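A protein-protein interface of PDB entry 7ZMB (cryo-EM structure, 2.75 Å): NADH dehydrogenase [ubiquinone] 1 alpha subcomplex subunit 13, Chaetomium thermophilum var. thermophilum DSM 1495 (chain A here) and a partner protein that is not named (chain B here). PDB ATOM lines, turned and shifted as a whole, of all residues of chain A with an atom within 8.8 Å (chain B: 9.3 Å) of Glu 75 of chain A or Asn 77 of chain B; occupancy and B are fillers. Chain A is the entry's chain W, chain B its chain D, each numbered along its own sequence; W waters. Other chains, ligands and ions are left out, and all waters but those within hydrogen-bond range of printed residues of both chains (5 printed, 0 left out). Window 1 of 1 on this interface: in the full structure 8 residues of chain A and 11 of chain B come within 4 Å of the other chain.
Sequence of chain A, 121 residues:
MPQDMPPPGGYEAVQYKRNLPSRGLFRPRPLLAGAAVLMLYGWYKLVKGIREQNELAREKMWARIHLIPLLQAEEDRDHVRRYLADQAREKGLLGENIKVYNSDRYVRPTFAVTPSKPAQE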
ATOM      1  N   ILE A  68      17.484  11.891 -14.396  1.00  0.00           N
ATOM      2  CA  ILE A  68      18.822  11.470 -14.899  1.00  0.00           C
ATOM      3  C   ILE A  68      19.226  12.209 -16.177  1.00  0.00           C
ATOM      4  O   ILE A  68      20.383  12.650 -16.211  1.00  0.00           O
ATOM      5  CB  ILE A  68      18.888   9.932 -15.059  1.00  0.00           C
ATOM      6  CG1 ILE A  68      19.213   9.214 -13.749  1.00  0.00           C
ATOM      7  CG2 ILE A  68      19.838   9.519 -16.171  1.00  0.00           C
ATOM      8  CD1 ILE A  68      19.250   7.711 -13.870  1.00  0.00           C
ATOM      9  N   PRO A  69      18.404  12.394 -17.241  1.00  0.00           N
ATOM     10  CA  PRO A  69      18.930  12.971 -18.488  1.00  0.00           C
ATOM     11  C   PRO A  69      19.237  14.466 -18.446  1.00  0.00           C
ATOM     12  O   PRO A  69      20.184  14.838 -19.052  1.00  0.00           O
ATOM     13  CB  PRO A  69      17.867  12.659 -19.551  1.00  0.00           C
ATOM     14  CG  PRO A  69      17.060  11.551 -18.915  1.00  0.00           C
ATOM     15  CD  PRO A  69      17.039  11.914 -17.446  1.00  0.00           C
ATOM     16  N   LEU A  70      18.462  15.251 -17.702  1.00  0.00           N
ATOM     17  CA  LEU A  70      18.741  16.705 -17.558  1.00  0.00           C
ATOM     18  C   LEU A  70      19.921  16.932 -16.615  1.00  0.00           C
ATOM     19  O   LEU A  70      20.634  17.929 -16.807  1.00  0.00           O
ATOM     20  CB  LEU A  70      17.470  17.429 -17.106  1.00  0.00           C
ATOM     21  CG  LEU A  70      16.819  16.931 -15.817  1.00  0.00           C
ATOM     22  CD1 LEU A  70      17.123  17.862 -14.652  1.00  0.00           C
ATOM     23  CD2 LEU A  70      15.315  16.792 -15.992  1.00  0.00           C
ATOM     24  N   LEU A  71      20.149  16.017 -15.676  1.00  0.00           N
ATOM     25  CA  LEU A  71      21.320  16.095 -14.758  1.00  0.00           C
ATOM     26  C   LEU A  71      22.575  15.643 -15.508  1.00  0.00           C
ATOM     27  O   LEU A  71      23.587  16.322 -15.396  1.00  0.00           O
ATOM     28  CB  LEU A  71      21.038  15.280 -13.497  1.00  0.00           C
ATOM     29  CG  LEU A  71      20.015  15.864 -12.525  1.00  0.00           C
ATOM     30  CD1 LEU A  71      19.569  14.812 -11.530  1.00  0.00           C
ATOM     31  CD2 LEU A  71      20.569  17.072 -11.795  1.00  0.00           C
ATOM     32  N   GLN A  72      22.515  14.506 -16.199  1.00  0.00           N
ATOM     33  CA  GLN A  72      23.667  13.990 -16.982  1.00  0.00           C
ATOM     34  C   GLN A  72      23.928  14.873 -18.202  1.00  0.00           C
ATOM     35  O   GLN A  72      25.044  14.852 -18.695  1.00  0.00           O
ATOM     36  CB  GLN A  72      23.517  12.503 -17.305  1.00  0.00           C
ATOM     37  CG  GLN A  72      24.796  11.833 -17.784  1.00  0.00           C
ATOM     38  CD  GLN A  72      25.911  11.808 -16.764  1.00  0.00           C
ATOM     39  OE1 GLN A  72      25.715  12.057 -15.578  1.00  0.00           O
ATOM     40  NE2 GLN A  72      27.109  11.490 -17.225  1.00  0.00           N
ATOM     41  N   ALA A  73      22.969  15.691 -18.611  1.00  0.00           N
ATOM     42  CA  ALA A  73      23.206  16.619 -19.739  1.00  0.00           C
ATOM     43  C   ALA A  73      24.026  17.806 -19.232  1.00  0.00           C
ATOM     44  O   ALA A  73      24.929  18.234 -19.961  1.00  0.00           O
ATOM     45  CB  ALA A  73      21.877  17.096 -20.244  1.00  0.00           C
ATOM     46  N   GLU A  74      23.744  18.277 -18.022  1.00  0.00           N
ATOM     47  CA  GLU A  74      24.505  19.378 -17.385  1.00  0.00           C
ATOM     48  C   GLU A  74      25.924  18.910 -17.060  1.00  0.00           C
ATOM     49  O   GLU A  74      26.861  19.704 -17.248  1.00  0.00           O
ATOM     50  CB  GLU A  74      23.776  19.765 -16.103  1.00  0.00           C
ATOM     51  CG  GLU A  74      24.437  20.880 -15.323  1.00  0.00           C
ATOM     52  CD  GLU A  74      24.009  20.922 -13.869  1.00  0.00           C
ATOM     53  OE1 GLU A  74      24.725  21.536 -13.065  1.00  0.00           O
ATOM     54  OE2 GLU A  74      22.966  20.328 -13.546  1.00  0.00           O
ATOM     55  N   GLU A  75      26.067  17.672 -16.574  1.00  0.00           N
ATOM     56  CA  GLU A  75      27.397  17.120 -16.215  1.00  0.00           C
ATOM     57  C   GLU A  75      28.267  17.006 -17.467  1.00  0.00           C
ATOM     58  O   GLU A  75      29.461  17.306 -17.380  1.00  0.00           O
ATOM     59  CB  GLU A  75      27.228  15.790 -15.480  1.00  0.00           C
ATOM     60  CG  GLU A  75      28.477  15.355 -14.746  1.00  0.00           C
ATOM     61  CD  GLU A  75      28.960  16.328 -13.684  1.00  0.00           C
ATOM     62  OE1 GLU A  75      28.106  16.934 -13.003  1.00  0.00           O
ATOM     63  OE2 GLU A  75      30.185  16.479 -13.541  1.00  0.00           O
ATOM     64  N   ASP A  76      27.682  16.571 -18.580  1.00  0.00           N
ATOM     65  CA  ASP A  76      28.430  16.411 -19.855  1.00  0.00           C
ATOM     66  C   ASP A  76      28.898  17.770 -20.370  1.00  0.00           C
ATOM     67  O   ASP A  76      30.030  17.848 -20.843  1.00  0.00           O
ATOM     68  CB  ASP A  76      27.602  15.680 -20.906  1.00  0.00           C
ATOM     69  CG  ASP A  76      27.319  14.226 -20.573  1.00  0.00           C
ATOM     70  OD1 ASP A  76      27.586  13.816 -19.428  1.00  0.00           O
ATOM     71  OD2 ASP A  76      26.842  13.514 -21.469  1.00  0.00           O
ATOM     72  N   ARG A  77      28.060  18.800 -20.252  1.00  0.00           N
ATOM     73  CA  ARG A  77      28.464  20.155 -20.692  1.00  0.00           C
ATOM     74  C   ARG A  77      29.661  20.603 -19.856  1.00  0.00           C
ATOM     75  O   ARG A  77      30.591  21.163 -20.438  1.00  0.00           O
ATOM     76  CB  ARG A  77      27.273  21.116 -20.664  1.00  0.00           C
ATOM     77  CG  ARG A  77      26.358  21.006 -21.871  1.00  0.00           C
ATOM     78  CD  ARG A  77      25.268  22.051 -21.784  1.00  0.00           C
ATOM     79  NE  ARG A  77      24.344  21.793 -20.694  1.00  0.00           N
ATOM     80  CZ  ARG A  77      23.162  21.210 -20.836  1.00  0.00           C
ATOM     81  NH1 ARG A  77      22.751  20.829 -22.031  1.00  0.00           N
ATOM     82  NH2 ARG A  77      22.390  21.021 -19.784  1.00  0.00           N
ATOM     83  N   ASP A  78      29.643  20.331 -18.553  1.00  0.00           N
ATOM     84  CA  ASP A  78      30.785  20.660 -17.659  1.00  0.00           C
ATOM     85  C   ASP A  78      32.023  19.854 -18.066  1.00  0.00           C
ATOM     86  O   ASP A  78      33.109  20.446 -18.107  1.00  0.00           O
ATOM     87  CB  ASP A  78      30.390  20.371 -16.210  1.00  0.00           C
ATOM     88  CG  ASP A  78      31.491  20.622 -15.200  1.00  0.00           C
ATOM     89  OD1 ASP A  78      31.869  21.793 -15.032  1.00  0.00           O
ATOM     90  OD2 ASP A  78      31.954  19.641 -14.586  1.00  0.00           O
ATOM     91  N   HIS A  79      31.860  18.564 -18.368  1.00  0.00           N
ATOM     92  CA  HIS A  79      32.997  17.675 -18.730  1.00  0.00           C
ATOM     93  C   HIS A  79      33.622  18.122 -20.046  1.00  0.00           C
ATOM     94  O   HIS A  79      34.858  18.086 -20.141  1.00  0.00           O
ATOM     95  CB  HIS A  79      32.561  16.202 -18.719  1.00  0.00           C
ATOM     96  CG  HIS A  79      32.616  15.600 -17.359  1.00  0.00           C
ATOM     97  ND1 HIS A  79      33.555  14.656 -17.011  1.00  0.00           N
ATOM     98  CD2 HIS A  79      31.878  15.826 -16.253  1.00  0.00           C
ATOM     99  CE1 HIS A  79      33.378  14.310 -15.756  1.00  0.00           C
ATOM    100  NE2 HIS A  79      32.357  15.014 -15.268  1.00  0.00           N
ATOM    101  N   VAL A  80      32.794  18.559 -20.994  1.00  0.00           N
ATOM    102  CA  VAL A  80      33.295  18.943 -22.337  1.00  0.00           C
ATOM    103  C   VAL A  80      33.863  20.347 -22.190  1.00  0.00           C
ATOM    104  O   VAL A  80      34.942  20.597 -22.746  1.00  0.00           O
ATOM    105  CB  VAL A  80      32.133  18.908 -23.352  1.00  0.00           C
ATOM    106  CG1 VAL A  80      32.446  19.646 -24.644  1.00  0.00           C
ATOM    107  CG2 VAL A  80      31.658  17.493 -23.635  1.00  0.00           C
ATOM    108  N   ARG A  81      33.220  21.187 -21.379  1.00  0.00           N
ATOM    109  CA  ARG A  81      33.790  22.532 -21.101  1.00  0.00           C
ATOM    110  C   ARG A  81      35.181  22.437 -20.476  1.00  0.00           C
ATOM    111  O   ARG A  81      36.031  23.236 -20.867  1.00  0.00           O
ATOM    112  CB  ARG A  81      32.873  23.298 -20.155  1.00  0.00           C
ATOM    113  CG  ARG A  81      33.164  24.785 -20.050  1.00  0.00           C
ATOM    114  CD  ARG A  81      32.209  25.450 -19.081  1.00  0.00           C
ATOM    115  NE  ARG A  81      32.157  24.779 -17.791  1.00  0.00           N
ATOM    116  CZ  ARG A  81      33.068  24.912 -16.839  1.00  0.00           C
ATOM    117  NH1 ARG A  81      32.937  24.269 -15.694  1.00  0.00           N
ATOM    118  NH2 ARG A  81      34.122  25.677 -17.042  1.00  0.00           N
ATOM    119  N   ARG A  82      35.447  21.445 -19.623  1.00  0.00           N
ATOM    120  CA  ARG A  82      36.792  21.432 -18.994  1.00  0.00           C
ATOM    121  C   ARG A  82      37.799  20.681 -19.847  1.00  0.00           C
ATOM    122  O   ARG A  82      38.982  20.998 -19.740  1.00  0.00           O
ATOM    123  CB  ARG A  82      36.714  20.932 -17.546  1.00  0.00           C
ATOM    124  CG  ARG A  82      35.779  21.755 -16.671  1.00  0.00           C
ATOM    125  CD  ARG A  82      35.714  21.383 -15.205  1.00  0.00           C
ATOM    126  NE  ARG A  82      36.991  21.537 -14.531  1.00  0.00           N
ATOM    127  CZ  ARG A  82      37.142  21.669 -13.220  1.00  0.00           C
ATOM    128  NH1 ARG A  82      38.352  21.795 -12.707  1.00  0.00           N
ATOM    129  NH2 ARG A  82      36.087  21.686 -12.430  1.00  0.00           N
ATOM    130  N   TYR A 106      36.390   9.787 -24.975  1.00  0.00           N
ATOM    131  CA  TYR A 106      36.648  10.680 -23.826  1.00  0.00           C
ATOM    132  C   TYR A 106      36.839   9.832 -22.575  1.00  0.00           C
ATOM    133  O   TYR A 106      36.033   8.918 -22.333  1.00  0.00           O
ATOM    134  CB  TYR A 106      35.474  11.625 -23.584  1.00  0.00           C
ATOM    135  CG  TYR A 106      35.592  12.404 -22.300  1.00  0.00           C
ATOM    136  CD1 TYR A 106      36.601  13.336 -22.128  1.00  0.00           C
ATOM    137  CD2 TYR A 106      34.719  12.190 -21.248  1.00  0.00           C
ATOM    138  CE1 TYR A 106      36.736  14.044 -20.950  1.00  0.00           C
ATOM    139  CE2 TYR A 106      34.838  12.893 -20.062  1.00  0.00           C
ATOM    140  CZ  TYR A 106      35.850  13.824 -19.914  1.00  0.00           C
ATOM    141  OH  TYR A 106      35.981  14.531 -18.757  1.00  0.00           O
ATOM    142  N   ARG A 108      37.143  10.187 -18.395  1.00  0.00           N
ATOM    143  CA  ARG A 108      37.029  11.063 -17.202  1.00  0.00           C
ATOM    144  C   ARG A 108      38.404  11.241 -16.524  1.00  0.00           C
ATOM    145  O   ARG A 108      38.890  10.244 -15.960  1.00  0.00           O
ATOM    146  CB  ARG A 108      35.896  10.543 -16.314  1.00  0.00           C
ATOM    147  CG  ARG A 108      34.527  11.002 -16.782  1.00  0.00           C
ATOM    148  CD  ARG A 108      33.430  10.130 -16.227  1.00  0.00           C
ATOM    149  NE  ARG A 108      32.115  10.555 -16.672  1.00  0.00           N
ATOM    150  CZ  ARG A 108      31.479  10.051 -17.721  1.00  0.00           C
ATOM    151  NH1 ARG A 108      30.278  10.492 -18.042  1.00  0.00           N
ATOM    152  NH2 ARG A 108      32.047   9.103 -18.444  1.00  0.00           N
ATOM    153  N   GLN B  48      25.217  13.795  -3.948  1.00  0.00           N
ATOM    154  CA  GLN B  48      25.421  14.647  -5.149  1.00  0.00           C
ATOM    155  C   GLN B  48      24.342  15.728  -5.231  1.00  0.00           C
ATOM    156  O   GLN B  48      24.689  16.866  -5.545  1.00  0.00           O
ATOM    157  CB  GLN B  48      25.411  13.779  -6.408  1.00  0.00           C
ATOM    158  CG  GLN B  48      26.667  12.962  -6.628  1.00  0.00           C
ATOM    159  CD  GLN B  48      26.534  12.162  -7.898  1.00  0.00           C
ATOM    160  OE1 GLN B  48      25.684  12.442  -8.737  1.00  0.00           O
ATOM    161  NE2 GLN B  48      27.392  11.169  -8.059  1.00  0.00           N
ATOM    162  N   GLU B  51      24.955  18.557  -2.886  1.00  0.00           N
ATOM    163  CA  GLU B  51      26.075  19.426  -3.303  1.00  0.00           C
ATOM    164  C   GLU B  51      25.546  20.312  -4.424  1.00  0.00           C
ATOM    165  O   GLU B  51      26.020  21.448  -4.538  1.00  0.00           O
ATOM    166  CB  GLU B  51      27.231  18.573  -3.808  1.00  0.00           C
ATOM    167  CG  GLU B  51      28.004  17.874  -2.711  1.00  0.00           C
ATOM    168  CD  GLU B  51      28.894  16.765  -3.243  1.00  0.00           C
ATOM    169  OE1 GLU B  51      28.548  16.193  -4.294  1.00  0.00           O
ATOM    170  OE2 GLU B  51      29.934  16.489  -2.616  1.00  0.00           O
ATOM    171  N   ARG B  52      24.526  19.836  -5.135  1.00  0.00           N
ATOM    172  CA  ARG B  52      23.949  20.640  -6.235  1.00  0.00           C
ATOM    173  C   ARG B  52      23.009  21.690  -5.628  1.00  0.00           C
ATOM    174  O   ARG B  52      22.683  22.646  -6.329  1.00  0.00           O
ATOM    175  CB  ARG B  52      23.325  19.745  -7.312  1.00  0.00           C
ATOM    176  CG  ARG B  52      23.196  20.435  -8.661  1.00  0.00           C
ATOM    177  CD  ARG B  52      22.494  19.625  -9.729  1.00  0.00           C
ATOM    178  NE  ARG B  52      21.919  20.513 -10.728  1.00  0.00           N
ATOM    179  CZ  ARG B  52      20.676  20.974 -10.693  1.00  0.00           C
ATOM    180  NH1 ARG B  52      19.863  20.616  -9.714  1.00  0.00           N
ATOM    181  NH2 ARG B  52      20.245  21.784 -11.642  1.00  0.00           N
ATOM    182  N   ASP B  53      22.685  21.567  -4.342  1.00  0.00           N
ATOM    183  CA  ASP B  53      21.828  22.570  -3.655  1.00  0.00           C
ATOM    184  C   ASP B  53      22.759  23.672  -3.161  1.00  0.00           C
ATOM    185  O   ASP B  53      22.374  24.840  -3.238  1.00  0.00           O
ATOM    186  CB  ASP B  53      21.021  21.935  -2.522  1.00  0.00           C
ATOM    187  CG  ASP B  53      19.895  21.040  -3.005  1.00  0.00           C
ATOM    188  OD1 ASP B  53      19.750  20.891  -4.230  1.00  0.00           O
ATOM    189  OD2 ASP B  53      19.176  20.502  -2.149  1.00  0.00           O
ATOM    190  N   ARG B  54      23.943  23.293  -2.685  1.00  0.00           N
ATOM    191  CA  ARG B  54      24.979  24.285  -2.302  1.00  0.00           C
ATOM    192  C   ARG B  54      25.355  25.109  -3.531  1.00  0.00           C
ATOM    193  O   ARG B  54      25.561  26.313  -3.378  1.00  0.00           O
ATOM    194  CB  ARG B  54      26.181  23.557  -1.707  1.00  0.00           C
ATOM    195  CG  ARG B  54      27.121  24.445  -0.911  1.00  0.00           C
ATOM    196  CD  ARG B  54      28.504  23.836  -0.843  1.00  0.00           C
ATOM    197  NE  ARG B  54      28.725  22.969   0.301  1.00  0.00           N
ATOM    198  CZ  ARG B  54      29.718  22.098   0.387  1.00  0.00           C
ATOM    199  NH1 ARG B  54      29.864  21.359   1.472  1.00  0.00           N
ATOM    200  NH2 ARG B  54      30.558  21.960  -0.622  1.00  0.00           N
ATOM    201  N   ARG B  55      25.427  24.483  -4.704  1.00  0.00           N
ATOM    202  CA  ARG B  55      25.757  25.199  -5.957  1.00  0.00           C
ATOM    203  C   ARG B  55      24.715  26.279  -6.276  1.00  0.00           C
ATOM    204  O   ARG B  55      25.094  27.274  -6.903  1.00  0.00           O
ATOM    205  CB  ARG B  55      25.954  24.211  -7.106  1.00  0.00           C
ATOM    206  CG  ARG B  55      27.201  23.350  -6.999  1.00  0.00           C
ATOM    207  CD  ARG B  55      27.134  22.352  -8.130  1.00  0.00           C
ATOM    208  NE  ARG B  55      27.129  23.040  -9.408  1.00  0.00           N
ATOM    209  CZ  ARG B  55      26.788  22.481 -10.558  1.00  0.00           C
ATOM    210  NH1 ARG B  55      26.411  21.216 -10.591  1.00  0.00           N
ATOM    211  NH2 ARG B  55      26.824  23.190 -11.670  1.00  0.00           N
ATOM    212  N   LEU B  56      23.461  26.085  -5.867  1.00  0.00           N
ATOM    213  CA  LEU B  56      22.384  27.066  -6.159  1.00  0.00           C
ATOM    214  C   LEU B  56      22.061  27.954  -4.949  1.00  0.00           C
ATOM    215  O   LEU B  56      21.499  29.024  -5.174  1.00  0.00           O
ATOM    216  CB  LEU B  56      21.143  26.296  -6.612  1.00  0.00           C
ATOM    217  CG  LEU B  56      21.265  25.488  -7.900  1.00  0.00           C
ATOM    218  CD1 LEU B  56      20.445  24.212  -7.830  1.00  0.00           C
ATOM    219  CD2 LEU B  56      20.842  26.319  -9.095  1.00  0.00           C
ATOM    220  N   GLY B  72      26.839  31.829 -13.508  1.00  0.00           N
ATOM    221  CA  GLY B  72      28.069  31.309 -12.876  1.00  0.00           C
ATOM    222  C   GLY B  72      27.852  29.928 -12.306  1.00  0.00           C
ATOM    223  O   GLY B  72      28.807  29.391 -11.731  1.00  0.00           O
ATOM    224  N   PHE B  73      26.657  29.370 -12.481  1.00  0.00           N
ATOM    225  CA  PHE B  73      26.340  28.007 -11.983  1.00  0.00           C
ATOM    226  C   PHE B  73      27.035  27.010 -12.906  1.00  0.00           C
ATOM    227  O   PHE B  73      27.403  25.910 -12.454  1.00  0.00           O
ATOM    228  CB  PHE B  73      24.826  27.828 -11.894  1.00  0.00           C
ATOM    229  CG  PHE B  73      24.353  26.441 -11.550  1.00  0.00           C
ATOM    230  CD1 PHE B  73      24.375  25.986 -10.242  1.00  0.00           C
ATOM    231  CD2 PHE B  73      23.864  25.598 -12.535  1.00  0.00           C
ATOM    232  CE1 PHE B  73      23.931  24.712  -9.930  1.00  0.00           C
ATOM    233  CE2 PHE B  73      23.416  24.328 -12.217  1.00  0.00           C
ATOM    234  CZ  PHE B  73      23.451  23.887 -10.917  1.00  0.00           C
ATOM    235  N   GLU B  74      27.276  27.423 -14.147  1.00  0.00           N
ATOM    236  CA  GLU B  74      27.946  26.556 -15.135  1.00  0.00           C
ATOM    237  C   GLU B  74      29.428  26.409 -14.758  1.00  0.00           C
ATOM    238  O   GLU B  74      30.105  25.584 -15.375  1.00  0.00           O
ATOM    239  CB  GLU B  74      27.719  27.177 -16.507  1.00  0.00           C
ATOM    240  CG  GLU B  74      27.585  28.685 -16.462  1.00  0.00           C
ATOM    241  CD  GLU B  74      27.210  29.324 -17.786  1.00  0.00           C
ATOM    242  OE1 GLU B  74      26.729  30.471 -17.769  1.00  0.00           O
ATOM    243  OE2 GLU B  74      27.401  28.670 -18.832  1.00  0.00           O
ATOM    244  N   PHE B  75      29.906  27.190 -13.783  1.00  0.00           N
ATOM    245  CA  PHE B  75      31.341  27.187 -13.407  1.00  0.00           C
ATOM    246  C   PHE B  75      31.588  26.707 -11.976  1.00  0.00           C
ATOM    247  O   PHE B  75      32.721  26.302 -11.727  1.00  0.00           O
ATOM    248  CB  PHE B  75      31.888  28.603 -13.568  1.00  0.00           C
ATOM    249  CG  PHE B  75      31.746  29.168 -14.958  1.00  0.00           C
ATOM    250  CD1 PHE B  75      30.713  30.032 -15.275  1.00  0.00           C
ATOM    251  CD2 PHE B  75      32.651  28.835 -15.950  1.00  0.00           C
ATOM    252  CE1 PHE B  75      30.597  30.561 -16.549  1.00  0.00           C
ATOM    253  CE2 PHE B  75      32.528  29.358 -17.226  1.00  0.00           C
ATOM    254  CZ  PHE B  75      31.504  30.221 -17.523  1.00  0.00           C
ATOM    255  N   ASN B  76      30.608  26.733 -11.073  1.00  0.00           N
ATOM    256  CA  ASN B  76      30.902  26.361  -9.695  1.00  0.00           C
ATOM    257  C   ASN B  76      30.808  24.868  -9.445  1.00  0.00           C
ATOM    258  O   ASN B  76      30.919  24.449  -8.291  1.00  0.00           O
ATOM    259  CB  ASN B  76      29.964  27.096  -8.728  1.00  0.00           C
ATOM    260  CG  ASN B  76      28.497  26.943  -9.094  1.00  0.00           C
ATOM    261  OD1 ASN B  76      28.080  25.920  -9.624  1.00  0.00           O
ATOM    262  ND2 ASN B  76      27.710  27.966  -8.807  1.00  0.00           N
ATOM    263  N   ASN B  77      30.583  24.062 -10.491  1.00  0.00           N
ATOM    264  CA  ASN B  77      30.444  22.588 -10.309  1.00  0.00           C
ATOM    265  C   ASN B  77      31.725  22.098  -9.654  1.00  0.00           C
ATOM    266  O   ASN B  77      32.781  22.205 -10.285  1.00  0.00           O
ATOM    267  CB  ASN B  77      30.144  21.840 -11.609  1.00  0.00           C
ATOM    268  CG  ASN B  77      29.725  20.402 -11.397  1.00  0.00           C
ATOM    269  OD1 ASN B  77      29.250  20.036 -10.326  1.00  0.00           O
ATOM    270  ND2 ASN B  77      29.880  19.580 -12.422  1.00  0.00           N
ATOM    271  N   PRO B  78      31.691  21.559  -8.421  1.00  0.00           N
ATOM    272  CA  PRO B  78      32.931  21.214  -7.736  1.00  0.00           C
ATOM    273  C   PRO B  78      33.640  19.970  -8.278  1.00  0.00           C
ATOM    274  O   PRO B  78      32.969  19.005  -8.535  1.00  0.00           O
ATOM    275  CB  PRO B  78      32.439  20.974  -6.301  1.00  0.00           C
ATOM    276  CG  PRO B  78      31.032  20.460  -6.477  1.00  0.00           C
ATOM    277  CD  PRO B  78      30.490  21.257  -7.642  1.00  0.00           C
ATOM    278  N   TRP B  79      34.951  20.043  -8.484  1.00  0.00           N
ATOM    279  CA  TRP B  79      35.719  18.823  -8.847  1.00  0.00           C
ATOM    280  C   TRP B  79      36.571  18.514  -7.620  1.00  0.00           C
ATOM    281  O   TRP B  79      37.309  19.403  -7.197  1.00  0.00           O
ATOM    282  CB  TRP B  79      36.514  18.995 -10.140  1.00  0.00           C
ATOM    283  CG  TRP B  79      35.755  18.617 -11.374  1.00  0.00           C
ATOM    284  CD1 TRP B  79      34.403  18.512 -11.513  1.00  0.00           C
ATOM    285  CD2 TRP B  79      36.314  18.301 -12.662  1.00  0.00           C
ATOM    286  NE1 TRP B  79      34.081  18.147 -12.791  1.00  0.00           N
ATOM    287  CE2 TRP B  79      35.232  18.011 -13.519  1.00  0.00           C
ATOM    288  CE3 TRP B  79      37.615  18.234 -13.171  1.00  0.00           C
ATOM    289  CZ2 TRP B  79      35.416  17.662 -14.855  1.00  0.00           C
ATOM    290  CZ3 TRP B  79      37.796  17.886 -14.491  1.00  0.00           C
ATOM    291  CH2 TRP B  79      36.710  17.606 -15.320  1.00  0.00           C
ATOM    292  N   LYS B  80      36.488  17.307  -7.078  1.00  0.00           N
ATOM    293  CA  LYS B  80      37.122  17.022  -5.801  1.00  0.00           C
ATOM    294  C   LYS B  80      38.595  16.678  -6.000  1.00  0.00           C
ATOM    295  O   LYS B  80      38.957  15.946  -6.920  1.00  0.00           O
ATOM    296  CB  LYS B  80      36.396  15.867  -5.120  1.00  0.00           C
ATOM    297  CG  LYS B  80      34.941  16.161  -4.871  1.00  0.00           C
ATOM    298  CD  LYS B  80      34.735  17.258  -3.900  1.00  0.00           C
ATOM    299  CE  LYS B  80      33.266  17.398  -3.578  1.00  0.00           C
ATOM    300  NZ  LYS B  80      32.515  17.910  -4.748  1.00  0.00           N
HETATM  301  O   HOH W   1      31.312  16.915 -10.524  1.00  0.00           O
HETATM  302  O   HOH W   2      20.480  19.554 -14.011  1.00  0.00           O
HETATM  303  O   HOH W   3      33.213  21.424 -12.731  1.00  0.00           O
HETATM  304  O   HOH W   4      34.483  24.457 -12.323  1.00  0.00           O
HETATM  305  O   HOH W   5      27.317  19.485 -13.883  1.00  0.00           O
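Of chain B, only Asn 77 (3.2 Å) comes within 4 Å of Glu 75 of chain A.
Asn 77 of chain B touches three residues of chain A.
Printed residues of chain A within 4 Å of Trp 79 of chain B: Asp 78 and Arg 82.
Of the printed residues of chain A, Phe 75 of chain B touches Arg 81.
Of the printed residues of chain B, Glu 74 of chain A touches Arg 52, Arg 55 and Phe 73.
Printed residues of chain B within 4 Å of Leu 71 of chain A: Arg 52.
Printed residues of chain A within 4 Å of Phe 73 of chain B: Glu 74 (3.2 Å).
The nearest residue of chain A that does not touch Asn 77 of chain B is Glu 74 of chain A (5.4 Å).
The nearest printed residue of chain B that does not touch Arg 81 of chain A is Asn 77 of chain B (5.5 Å).
The guanidinium group (NH1) of Arg 55 of chain B is in hydrogen-bond range of the side-chain amide oxygen (OD1) of Asn 77 of chain B, at 3.1 Å.
OD1 of Asn 76 of chain B sits at hydrogen-bond distance from NE of Arg 55 of chain B, at 3.0 Å.
OE2 of Glu 75 of chain A sits at hydrogen-bond distance from NE2 of His 79 of chain A.
Of the 16 printed residues of chain B, 7 touch a printed residue of chain A.
Printed residues of chain B that touch a printed residue of chain A: Arg 52, Arg 55, Phe 73, Glu 74, Phe 75, Asn 77 and Trp 79.
Along chain B the printed residues that touch a printed residue of chain A span positions 52 to 79.
Of the 17 printed residues of chain A, 6 touch a printed residue of chain B.
Hydrophobic or aromatic side chains of chain A that line the printed part of chain B: Leu 71.
The side-chain amide nitrogen of Asn 77 of chain B is in hydrogen-bond range of the side-chain carboxylate of Glu 75 of chain A (3.2 Å).
NH1 of Arg 81 of chain A sits at hydrogen-bond distance from O of Glu 74 of chain B (3.1 Å).
The side-chain carboxylate (OD2) of Asp 78 of chain A lies within hydrogen-bond range of the indole nitrogen (NE1) of Trp 79 of chain B.
The side-chain carboxylate (OE2) of Glu 74 of chain A lies within salt-bridge range of the guanidinium group (NE) of Arg 52 of chain B (3.0 Å).
NH1 of Arg 55 of chain B lies within salt-bridge range of OE1 of Glu 74 of chain A.
The side-chain amide nitrogen (ND2) of Asn 77 of chain B sits at hydrogen-bond distance from the side-chain carboxylate (OD2) of Asp 78 of chain A (3.0 Å).
Arg 52 of chain B touches Leu 71 of chain A (CD to CD2, 3.8 Å).
Glu 74 of chain A touches Phe 73 of chain B (OE1 to CE2, 3.2 Å).
Arg 81 of chain A touches Phe 75 of chain B (NH2 to CD2, 3.7 Å).
NH2 of Arg 82 of chain A touches O of Asn 77 of chain B, at 3.97 Å.
Trp 79 of chain B touches Arg 82 of chain A.
Water W4 lies within hydrogen-bond range of O of Phe 75 of chain B (2.6 Å), NH2 of Arg 82 of chain A (3.2 Å) and O of Asn 77 of chain B (3.5 Å).
Water W2 lies within hydrogen-bond range of the side-chain carboxylate of Glu 74 of chain A (2.6 Å), the backbone carbonyl oxygen of Leu 70 of chain A (3.2 Å) and the guanidinium group of Arg 52 of chain B (3.3 Å).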
